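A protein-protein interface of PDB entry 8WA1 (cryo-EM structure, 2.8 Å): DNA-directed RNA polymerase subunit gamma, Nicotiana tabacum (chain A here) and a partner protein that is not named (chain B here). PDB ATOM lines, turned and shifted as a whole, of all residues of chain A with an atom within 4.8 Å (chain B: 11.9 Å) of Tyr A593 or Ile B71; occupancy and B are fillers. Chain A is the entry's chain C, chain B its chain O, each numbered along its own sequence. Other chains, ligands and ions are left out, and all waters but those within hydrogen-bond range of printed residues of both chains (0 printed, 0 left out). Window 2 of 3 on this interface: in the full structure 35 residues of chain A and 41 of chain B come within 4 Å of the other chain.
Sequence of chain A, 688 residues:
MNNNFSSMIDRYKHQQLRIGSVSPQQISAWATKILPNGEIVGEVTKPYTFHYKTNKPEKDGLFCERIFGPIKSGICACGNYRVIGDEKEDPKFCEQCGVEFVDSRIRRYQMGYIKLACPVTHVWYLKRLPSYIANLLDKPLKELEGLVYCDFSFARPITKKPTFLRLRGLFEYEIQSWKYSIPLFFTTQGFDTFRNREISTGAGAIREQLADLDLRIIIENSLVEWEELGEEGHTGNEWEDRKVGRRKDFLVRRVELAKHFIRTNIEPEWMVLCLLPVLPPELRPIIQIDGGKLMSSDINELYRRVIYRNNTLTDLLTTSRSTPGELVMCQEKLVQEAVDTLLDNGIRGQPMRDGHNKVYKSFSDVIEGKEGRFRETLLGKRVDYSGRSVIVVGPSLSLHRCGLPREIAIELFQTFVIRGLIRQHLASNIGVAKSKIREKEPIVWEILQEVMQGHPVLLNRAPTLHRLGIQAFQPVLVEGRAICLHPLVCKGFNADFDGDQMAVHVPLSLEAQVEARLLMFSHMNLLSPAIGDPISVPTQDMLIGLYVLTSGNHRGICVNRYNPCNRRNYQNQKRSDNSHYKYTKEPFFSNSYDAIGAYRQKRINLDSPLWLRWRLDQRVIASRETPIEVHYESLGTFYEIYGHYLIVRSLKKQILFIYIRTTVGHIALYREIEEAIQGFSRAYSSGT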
ATOM      1  N   ASN A 591      11.829 -30.808   6.308  1.00  0.00           N
ATOM      2  CA  ASN A 591      12.554 -30.348   7.480  1.00  0.00           C
ATOM      3  C   ASN A 591      12.940 -31.535   8.349  1.00  0.00           C
ATOM      4  O   ASN A 591      12.302 -32.590   8.320  1.00  0.00           O
ATOM      5  CB  ASN A 591      11.722 -29.349   8.298  1.00  0.00           C
ATOM      6  CG  ASN A 591      11.225 -28.186   7.466  1.00  0.00           C
ATOM      7  OD1 ASN A 591      10.021 -27.952   7.361  1.00  0.00           O
ATOM      8  ND2 ASN A 591      12.153 -27.449   6.867  1.00  0.00           N
ATOM      9  N   SER A 592      14.007 -31.346   9.130  1.00  0.00           N
ATOM     10  CA  SER A 592      14.425 -32.378  10.071  1.00  0.00           C
ATOM     11  C   SER A 592      13.410 -32.532  11.196  1.00  0.00           C
ATOM     12  O   SER A 592      13.240 -33.626  11.748  1.00  0.00           O
ATOM     13  CB  SER A 592      15.805 -32.042  10.636  1.00  0.00           C
ATOM     14  OG  SER A 592      16.703 -31.686   9.600  1.00  0.00           O
ATOM     15  N   TYR A 593      12.734 -31.437  11.552  1.00  0.00           N
ATOM     16  CA  TYR A 593      11.715 -31.496  12.593  1.00  0.00           C
ATOM     17  C   TYR A 593      10.581 -32.433  12.198  1.00  0.00           C
ATOM     18  O   TYR A 593      10.067 -33.182  13.035  1.00  0.00           O
ATOM     19  CB  TYR A 593      11.178 -30.092  12.875  1.00  0.00           C
ATOM     20  CG  TYR A 593      12.247 -29.020  12.897  1.00  0.00           C
ATOM     21  CD1 TYR A 593      12.996 -28.782  14.040  1.00  0.00           C
ATOM     22  CD2 TYR A 593      12.502 -28.245  11.773  1.00  0.00           C
ATOM     23  CE1 TYR A 593      13.973 -27.805  14.064  1.00  0.00           C
ATOM     24  CE2 TYR A 593      13.476 -27.265  11.788  1.00  0.00           C
ATOM     25  CZ  TYR A 593      14.208 -27.048  12.936  1.00  0.00           C
ATOM     26  OH  TYR A 593      15.179 -26.074  12.955  1.00  0.00           O
ATOM     27  N   ASP A 594      10.191 -32.417  10.921  1.00  0.00           N
ATOM     28  CA  ASP A 594       9.128 -33.301  10.460  1.00  0.00           C
ATOM     29  C   ASP A 594       9.544 -34.763  10.563  1.00  0.00           C
ATOM     30  O   ASP A 594       8.753 -35.613  10.990  1.00  0.00           O
ATOM     31  CB  ASP A 594       8.744 -32.953   9.022  1.00  0.00           C
ATOM     32  CG  ASP A 594       8.429 -31.482   8.845  1.00  0.00           C
ATOM     33  OD1 ASP A 594       7.927 -30.860   9.805  1.00  0.00           O
ATOM     34  OD2 ASP A 594       8.688 -30.946   7.748  1.00  0.00           O
ATOM     35  N   ALA A 595      10.785 -35.074  10.185  1.00  0.00           N
ATOM     36  CA  ALA A 595      11.259 -36.451  10.274  1.00  0.00           C
ATOM     37  C   ALA A 595      11.357 -36.912  11.723  1.00  0.00           C
ATOM     38  O   ALA A 595      11.002 -38.053  12.043  1.00  0.00           O
ATOM     39  CB  ALA A 595      12.609 -36.586   9.573  1.00  0.00           C
ATOM     40  N   ILE A 596      11.830 -36.039  12.616  1.00  0.00           N
ATOM     41  CA  ILE A 596      11.928 -36.414  14.024  1.00  0.00           C
ATOM     42  C   ILE A 596      10.540 -36.607  14.623  1.00  0.00           C
ATOM     43  O   ILE A 596      10.316 -37.523  15.424  1.00  0.00           O
ATOM     44  CB  ILE A 596      12.753 -35.372  14.801  1.00  0.00           C
ATOM     45  CG1 ILE A 596      14.212 -35.419  14.342  1.00  0.00           C
ATOM     46  CG2 ILE A 596      12.656 -35.613  16.300  1.00  0.00           C
ATOM     47  CD1 ILE A 596      15.153 -34.609  15.198  1.00  0.00           C
ATOM     48  N   GLY A 597       9.581 -35.766  14.231  1.00  0.00           N
ATOM     49  CA  GLY A 597       8.219 -35.955  14.699  1.00  0.00           C
ATOM     50  C   GLY A 597       7.599 -37.239  14.181  1.00  0.00           C
ATOM     51  O   GLY A 597       6.870 -37.922  14.902  1.00  0.00           O
ATOM     52  N   ARG A 671      21.271 -32.324  14.503  1.00  0.00           N
ATOM     53  CA  ARG A 671      20.385 -31.307  15.050  1.00  0.00           C
ATOM     54  C   ARG A 671      20.670 -31.058  16.521  1.00  0.00           C
ATOM     55  O   ARG A 671      20.628 -29.913  16.974  1.00  0.00           O
ATOM     56  CB  ARG A 671      18.923 -31.711  14.855  1.00  0.00           C
ATOM     57  CG  ARG A 671      17.942 -30.712  15.452  1.00  0.00           C
ATOM     58  CD  ARG A 671      16.521 -31.248  15.492  1.00  0.00           C
ATOM     59  NE  ARG A 671      15.640 -30.374  16.263  1.00  0.00           N
ATOM     60  CZ  ARG A 671      14.354 -30.617  16.491  1.00  0.00           C
ATOM     61  NH1 ARG A 671      13.785 -31.711  16.004  1.00  0.00           N
ATOM     62  NH2 ARG A 671      13.633 -29.763  17.204  1.00  0.00           N
ATOM     63  N   GLU A 674      23.920 -28.983  16.696  1.00  0.00           N
ATOM     64  CA  GLU A 674      23.681 -27.621  16.230  1.00  0.00           C
ATOM     65  C   GLU A 674      22.824 -26.843  17.221  1.00  0.00           C
ATOM     66  O   GLU A 674      23.090 -25.667  17.491  1.00  0.00           O
ATOM     67  CB  GLU A 674      23.024 -27.654  14.849  1.00  0.00           C
ATOM     68  CG  GLU A 674      23.224 -26.399  14.003  1.00  0.00           C
ATOM     69  CD  GLU A 674      22.308 -25.255  14.399  1.00  0.00           C
ATOM     70  OE1 GLU A 674      22.754 -24.364  15.149  1.00  0.00           O
ATOM     71  OE2 GLU A 674      21.139 -25.248  13.957  1.00  0.00           O
ATOM     72  N   GLN A 678      23.650 -23.445  19.260  1.00  0.00           N
ATOM     73  CA  GLN A 678      22.802 -22.267  19.119  1.00  0.00           C
ATOM     74  C   GLN A 678      22.187 -21.858  20.452  1.00  0.00           C
ATOM     75  O   GLN A 678      22.052 -20.664  20.734  1.00  0.00           O
ATOM     76  CB  GLN A 678      21.715 -22.524  18.077  1.00  0.00           C
ATOM     77  CG  GLN A 678      20.843 -21.315  17.789  1.00  0.00           C
ATOM     78  CD  GLN A 678      20.079 -21.448  16.489  1.00  0.00           C
ATOM     79  OE1 GLN A 678      20.382 -22.311  15.666  1.00  0.00           O
ATOM     80  NE2 GLN A 678      19.083 -20.592  16.297  1.00  0.00           N
ATOM     81  N   ARG A 682      22.670 -18.301  22.249  1.00  0.00           N
ATOM     82  CA  ARG A 682      21.524 -17.485  22.642  1.00  0.00           C
ATOM     83  C   ARG A 682      21.532 -17.202  24.138  1.00  0.00           C
ATOM     84  O   ARG A 682      21.212 -16.086  24.566  1.00  0.00           O
ATOM     85  CB  ARG A 682      20.223 -18.176  22.233  1.00  0.00           C
ATOM     86  CG  ARG A 682      19.949 -18.154  20.738  1.00  0.00           C
ATOM     87  CD  ARG A 682      18.727 -18.990  20.386  1.00  0.00           C
ATOM     88  NE  ARG A 682      17.535 -18.561  21.111  1.00  0.00           N
ATOM     89  CZ  ARG A 682      16.338 -19.126  20.981  1.00  0.00           C
ATOM     90  NH1 ARG A 682      16.173 -20.147  20.151  1.00  0.00           N
ATOM     91  NH2 ARG A 682      15.307 -18.672  21.679  1.00  0.00           N
ATOM     92  N   ARG B  70      16.709 -18.665  13.845  1.00  0.00           N
ATOM     93  CA  ARG B  70      16.150 -18.943  15.162  1.00  0.00           C
ATOM     94  C   ARG B  70      15.479 -20.315  15.181  1.00  0.00           C
ATOM     95  O   ARG B  70      14.467 -20.528  14.514  1.00  0.00           O
ATOM     96  CB  ARG B  70      15.146 -17.859  15.558  1.00  0.00           C
ATOM     97  CG  ARG B  70      14.826 -17.826  17.043  1.00  0.00           C
ATOM     98  CD  ARG B  70      15.993 -17.264  17.842  1.00  0.00           C
ATOM     99  NE  ARG B  70      16.300 -15.890  17.455  1.00  0.00           N
ATOM    100  CZ  ARG B  70      17.289 -15.170  17.974  1.00  0.00           C
ATOM    101  NH1 ARG B  70      18.074 -15.691  18.907  1.00  0.00           N
ATOM    102  NH2 ARG B  70      17.494 -13.926  17.559  1.00  0.00           N
ATOM    103  N   ILE B  71      16.051 -21.240  15.945  1.00  0.00           N
ATOM    104  CA  ILE B  71      15.473 -22.587  16.018  1.00  0.00           C
ATOM    105  C   ILE B  71      14.183 -22.536  16.826  1.00  0.00           C
ATOM    106  O   ILE B  71      14.117 -21.819  17.848  1.00  0.00           O
ATOM    107  CB  ILE B  71      16.483 -23.580  16.624  1.00  0.00           C
ATOM    108  CG1 ILE B  71      17.160 -24.395  15.517  1.00  0.00           C
ATOM    109  CG2 ILE B  71      15.815 -24.513  17.624  1.00  0.00           C
ATOM    110  CD1 ILE B  71      17.715 -23.564  14.374  1.00  0.00           C
ATOM    111  N   PRO B  72      13.128 -23.253  16.424  1.00  0.00           N
ATOM    112  CA  PRO B  72      11.820 -23.056  17.075  1.00  0.00           C
ATOM    113  C   PRO B  72      11.718 -23.669  18.460  1.00  0.00           C
ATOM    114  O   PRO B  72      10.959 -23.165  19.299  1.00  0.00           O
ATOM    115  CB  PRO B  72      10.840 -23.726  16.097  1.00  0.00           C
ATOM    116  CG  PRO B  72      11.629 -23.998  14.842  1.00  0.00           C
ATOM    117  CD  PRO B  72      13.040 -24.170  15.281  1.00  0.00           C
ATOM    118  N   PHE B  73      12.458 -24.743  18.734  1.00  0.00           N
ATOM    119  CA  PHE B  73      12.231 -25.578  19.913  1.00  0.00           C
ATOM    120  C   PHE B  73      13.468 -25.522  20.810  1.00  0.00           C
ATOM    121  O   PHE B  73      13.963 -26.545  21.287  1.00  0.00           O
ATOM    122  CB  PHE B  73      11.894 -27.014  19.505  1.00  0.00           C
ATOM    123  CG  PHE B  73      10.827 -27.107  18.452  1.00  0.00           C
ATOM    124  CD1 PHE B  73       9.492 -26.978  18.788  1.00  0.00           C
ATOM    125  CD2 PHE B  73      11.162 -27.320  17.124  1.00  0.00           C
ATOM    126  CE1 PHE B  73       8.509 -27.062  17.821  1.00  0.00           C
ATOM    127  CE2 PHE B  73      10.184 -27.405  16.154  1.00  0.00           C
ATOM    128  CZ  PHE B  73       8.856 -27.275  16.502  1.00  0.00           C
ATOM    129  N   LEU B  74      13.971 -24.309  21.034  1.00  0.00           N
ATOM    130  CA  LEU B  74      15.137 -24.099  21.880  1.00  0.00           C
ATOM    131  C   LEU B  74      14.824 -23.275  23.124  1.00  0.00           C
ATOM    132  O   LEU B  74      15.734 -22.657  23.688  1.00  0.00           O
ATOM    133  CB  LEU B  74      16.256 -23.429  21.078  1.00  0.00           C
ATOM    134  CG  LEU B  74      17.648 -24.031  21.264  1.00  0.00           C
ATOM    135  CD1 LEU B  74      17.591 -25.537  21.084  1.00  0.00           C
ATOM    136  CD2 LEU B  74      18.624 -23.413  20.280  1.00  0.00           C
ATOM    137  N   GLU B  75      13.565 -23.247  23.565  1.00  0.00           N
ATOM    138  CA  GLU B  75      13.220 -22.468  24.750  1.00  0.00           C
ATOM    139  C   GLU B  75      13.694 -23.158  26.025  1.00  0.00           C
ATOM    140  O   GLU B  75      14.371 -22.543  26.861  1.00  0.00           O
ATOM    141  CB  GLU B  75      11.710 -22.233  24.800  1.00  0.00           C
ATOM    142  CG  GLU B  75      11.043 -22.139  23.437  1.00  0.00           C
ATOM    143  CD  GLU B  75      11.492 -20.932  22.635  1.00  0.00           C
ATOM    144  OE1 GLU B  75      11.921 -19.932  23.247  1.00  0.00           O
ATOM    145  OE2 GLU B  75      11.417 -20.987  21.390  1.00  0.00           O
ATOM    146  N   GLU B  76      13.352 -24.439  26.186  1.00  0.00           N
ATOM    147  CA  GLU B  76      13.667 -25.142  27.425  1.00  0.00           C
ATOM    148  C   GLU B  76      15.170 -25.307  27.605  1.00  0.00           C
ATOM    149  O   GLU B  76      15.672 -25.270  28.732  1.00  0.00           O
ATOM    150  CB  GLU B  76      12.964 -26.502  27.445  1.00  0.00           C
ATOM    151  CG  GLU B  76      12.885 -27.157  28.819  1.00  0.00           C
ATOM    152  CD  GLU B  76      14.146 -27.915  29.188  1.00  0.00           C
ATOM    153  OE1 GLU B  76      14.922 -28.264  28.274  1.00  0.00           O
ATOM    154  OE2 GLU B  76      14.363 -28.161  30.393  1.00  0.00           O
ATOM    155  N   GLN B  77      15.907 -25.478  26.505  1.00  0.00           N
ATOM    156  CA  GLN B  77      17.356 -25.618  26.606  1.00  0.00           C
ATOM    157  C   GLN B  77      18.000 -24.349  27.153  1.00  0.00           C
ATOM    158  O   GLN B  77      18.819 -24.409  28.077  1.00  0.00           O
ATOM    159  CB  GLN B  77      17.947 -25.976  25.245  1.00  0.00           C
ATOM    160  CG  GLN B  77      19.463 -26.040  25.236  1.00  0.00           C
ATOM    161  CD  GLN B  77      20.020 -26.369  23.871  1.00  0.00           C
ATOM    162  OE1 GLN B  77      19.470 -27.197  23.146  1.00  0.00           O
ATOM    163  NE2 GLN B  77      21.115 -25.714  23.506  1.00  0.00           N
ATOM    164  N   VAL B  78      17.646 -23.190  26.591  1.00  0.00           N
ATOM    165  CA  VAL B  78      18.197 -21.929  27.081  1.00  0.00           C
ATOM    166  C   VAL B  78      17.743 -21.672  28.511  1.00  0.00           C
ATOM    167  O   VAL B  78      18.509 -21.166  29.343  1.00  0.00           O
ATOM    168  CB  VAL B  78      17.805 -20.772  26.141  1.00  0.00           C
ATOM    169  CG1 VAL B  78      18.335 -19.450  26.672  1.00  0.00           C
ATOM    170  CG2 VAL B  78      18.329 -21.027  24.738  1.00  0.00           C
ATOM    171  N   ARG B  79      16.493 -22.024  28.824  1.00  0.00           N
ATOM    172  CA  ARG B  79      15.997 -21.870  30.188  1.00  0.00           C
ATOM    173  C   ARG B  79      16.835 -22.680  31.170  1.00  0.00           C
ATOM    174  O   ARG B  79      17.217 -22.188  32.237  1.00  0.00           O
ATOM    175  CB  ARG B  79      14.532 -22.293  30.259  1.00  0.00           C
ATOM    176  CG  ARG B  79      13.862 -22.008  31.589  1.00  0.00           C
ATOM    177  CD  ARG B  79      12.659 -22.913  31.793  1.00  0.00           C
ATOM    178  NE  ARG B  79      11.995 -23.232  30.532  1.00  0.00           N
ATOM    179  CZ  ARG B  79      11.056 -22.481  29.968  1.00  0.00           C
ATOM    180  NH1 ARG B  79      10.664 -21.356  30.549  1.00  0.00           N
ATOM    181  NH2 ARG B  79      10.509 -22.853  28.818  1.00  0.00           N
ATOM    182  N   ILE B  81      19.913 -23.790  30.696  1.00  0.00           N
ATOM    183  CA  ILE B  81      21.267 -23.242  30.732  1.00  0.00           C
ATOM    184  C   ILE B  81      21.333 -22.055  31.685  1.00  0.00           C
ATOM    185  O   ILE B  81      22.283 -21.916  32.464  1.00  0.00           O
ATOM    186  CB  ILE B  81      21.732 -22.857  29.315  1.00  0.00           C
ATOM    187  CG1 ILE B  81      21.936 -24.108  28.460  1.00  0.00           C
ATOM    188  CG2 ILE B  81      23.018 -22.049  29.374  1.00  0.00           C
ATOM    189  CD1 ILE B  81      22.355 -23.807  27.038  1.00  0.00           C
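No residue of chain B comes within 4 Å of Asn A591. No residue of chain B comes within 4 Å of Ser A592. Tyr A593 touches just these residues of chain B: Ile B71, Pro B72 and Phe B73. No residue of chain B comes within 4 Å of Asp A594. No residue of chain B comes within 4 Å of Ala A595. No residue of chain B comes within 4 Å of Gly A597. Of the printed residues of chain B, Glu A674 touches Ile B71 (3.8 Å). Of chain B, only Arg B70, Ile B71 and Leu B74 come within 4 Å of Gln A678. Printed residues of chain A within 4 Å of Arg B70: Gln A678 (3.6 Å) and Arg A682 (3.6 Å). Ile B71 touches just these residues of chain A: Tyr A593, Glu A674, Gln A678 and Arg A682. Of the printed residues of chain A, Pro B72 touches Tyr A593. Of the printed residues of chain A, Phe B73 touches Tyr A593 and Arg A671. Of the printed residues of chain A, Glu B75 touches Arg A682. Arg B79 touches none of the printed residues of chain A. The nearest residue of chain B that does not touch Tyr A593 is Arg B70 (5.8 Å). The nearest printed residue of chain A that does not touch Ile B71 is Arg A671 (5.7 Å). The nearest printed residue of chain A that does not touch Phe B73 is Arg A682 (6.1 Å).
The backbone NH (N) of Ile B71 lies close to the side-chain amide nitrogen (NE2) of Gln A678, at 3.1 Å. OE1 of Glu B75 lies within salt-bridge range of NH2 of Arg A682.
Tyr A593 touches Ile B71 (OH to CG1, 3.6 Å). OH of Tyr A593 touches CD of Pro B72, 3.7 Å away. Tyr A593 touches Phe B73. Phe B73 touches Arg A671. OE2 of Glu A674 touches CD1 of Ile B71 (3.8 Å). CA of Arg B70 touches NE2 of Gln A678, at 3.6 Å. Gln A678 touches Leu B74 (C to CD2, 3.9 Å). Arg A682 touches Arg B70 (CG to NH1, 3.6 Å). NH1 of Arg A682 touches O of Ile B71, 3.5 Å away. Leu B74 touches Arg A682.
Of the 11 printed residues of chain A, 5 touch a printed residue of chain B. Printed residues of chain A that touch a printed residue of chain B: Tyr A593, Arg A671, Glu A674, Gln A678 and Arg A682. Hydrophobic or aromatic side chains of chain B that line the printed part of chain A: Ile B71, Pro B72, Phe B73 and Leu B74.
The side-chain carboxylate (OE1) of Glu A674 sits close to the side-chain amide oxygen (OE1) of Gln A678.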
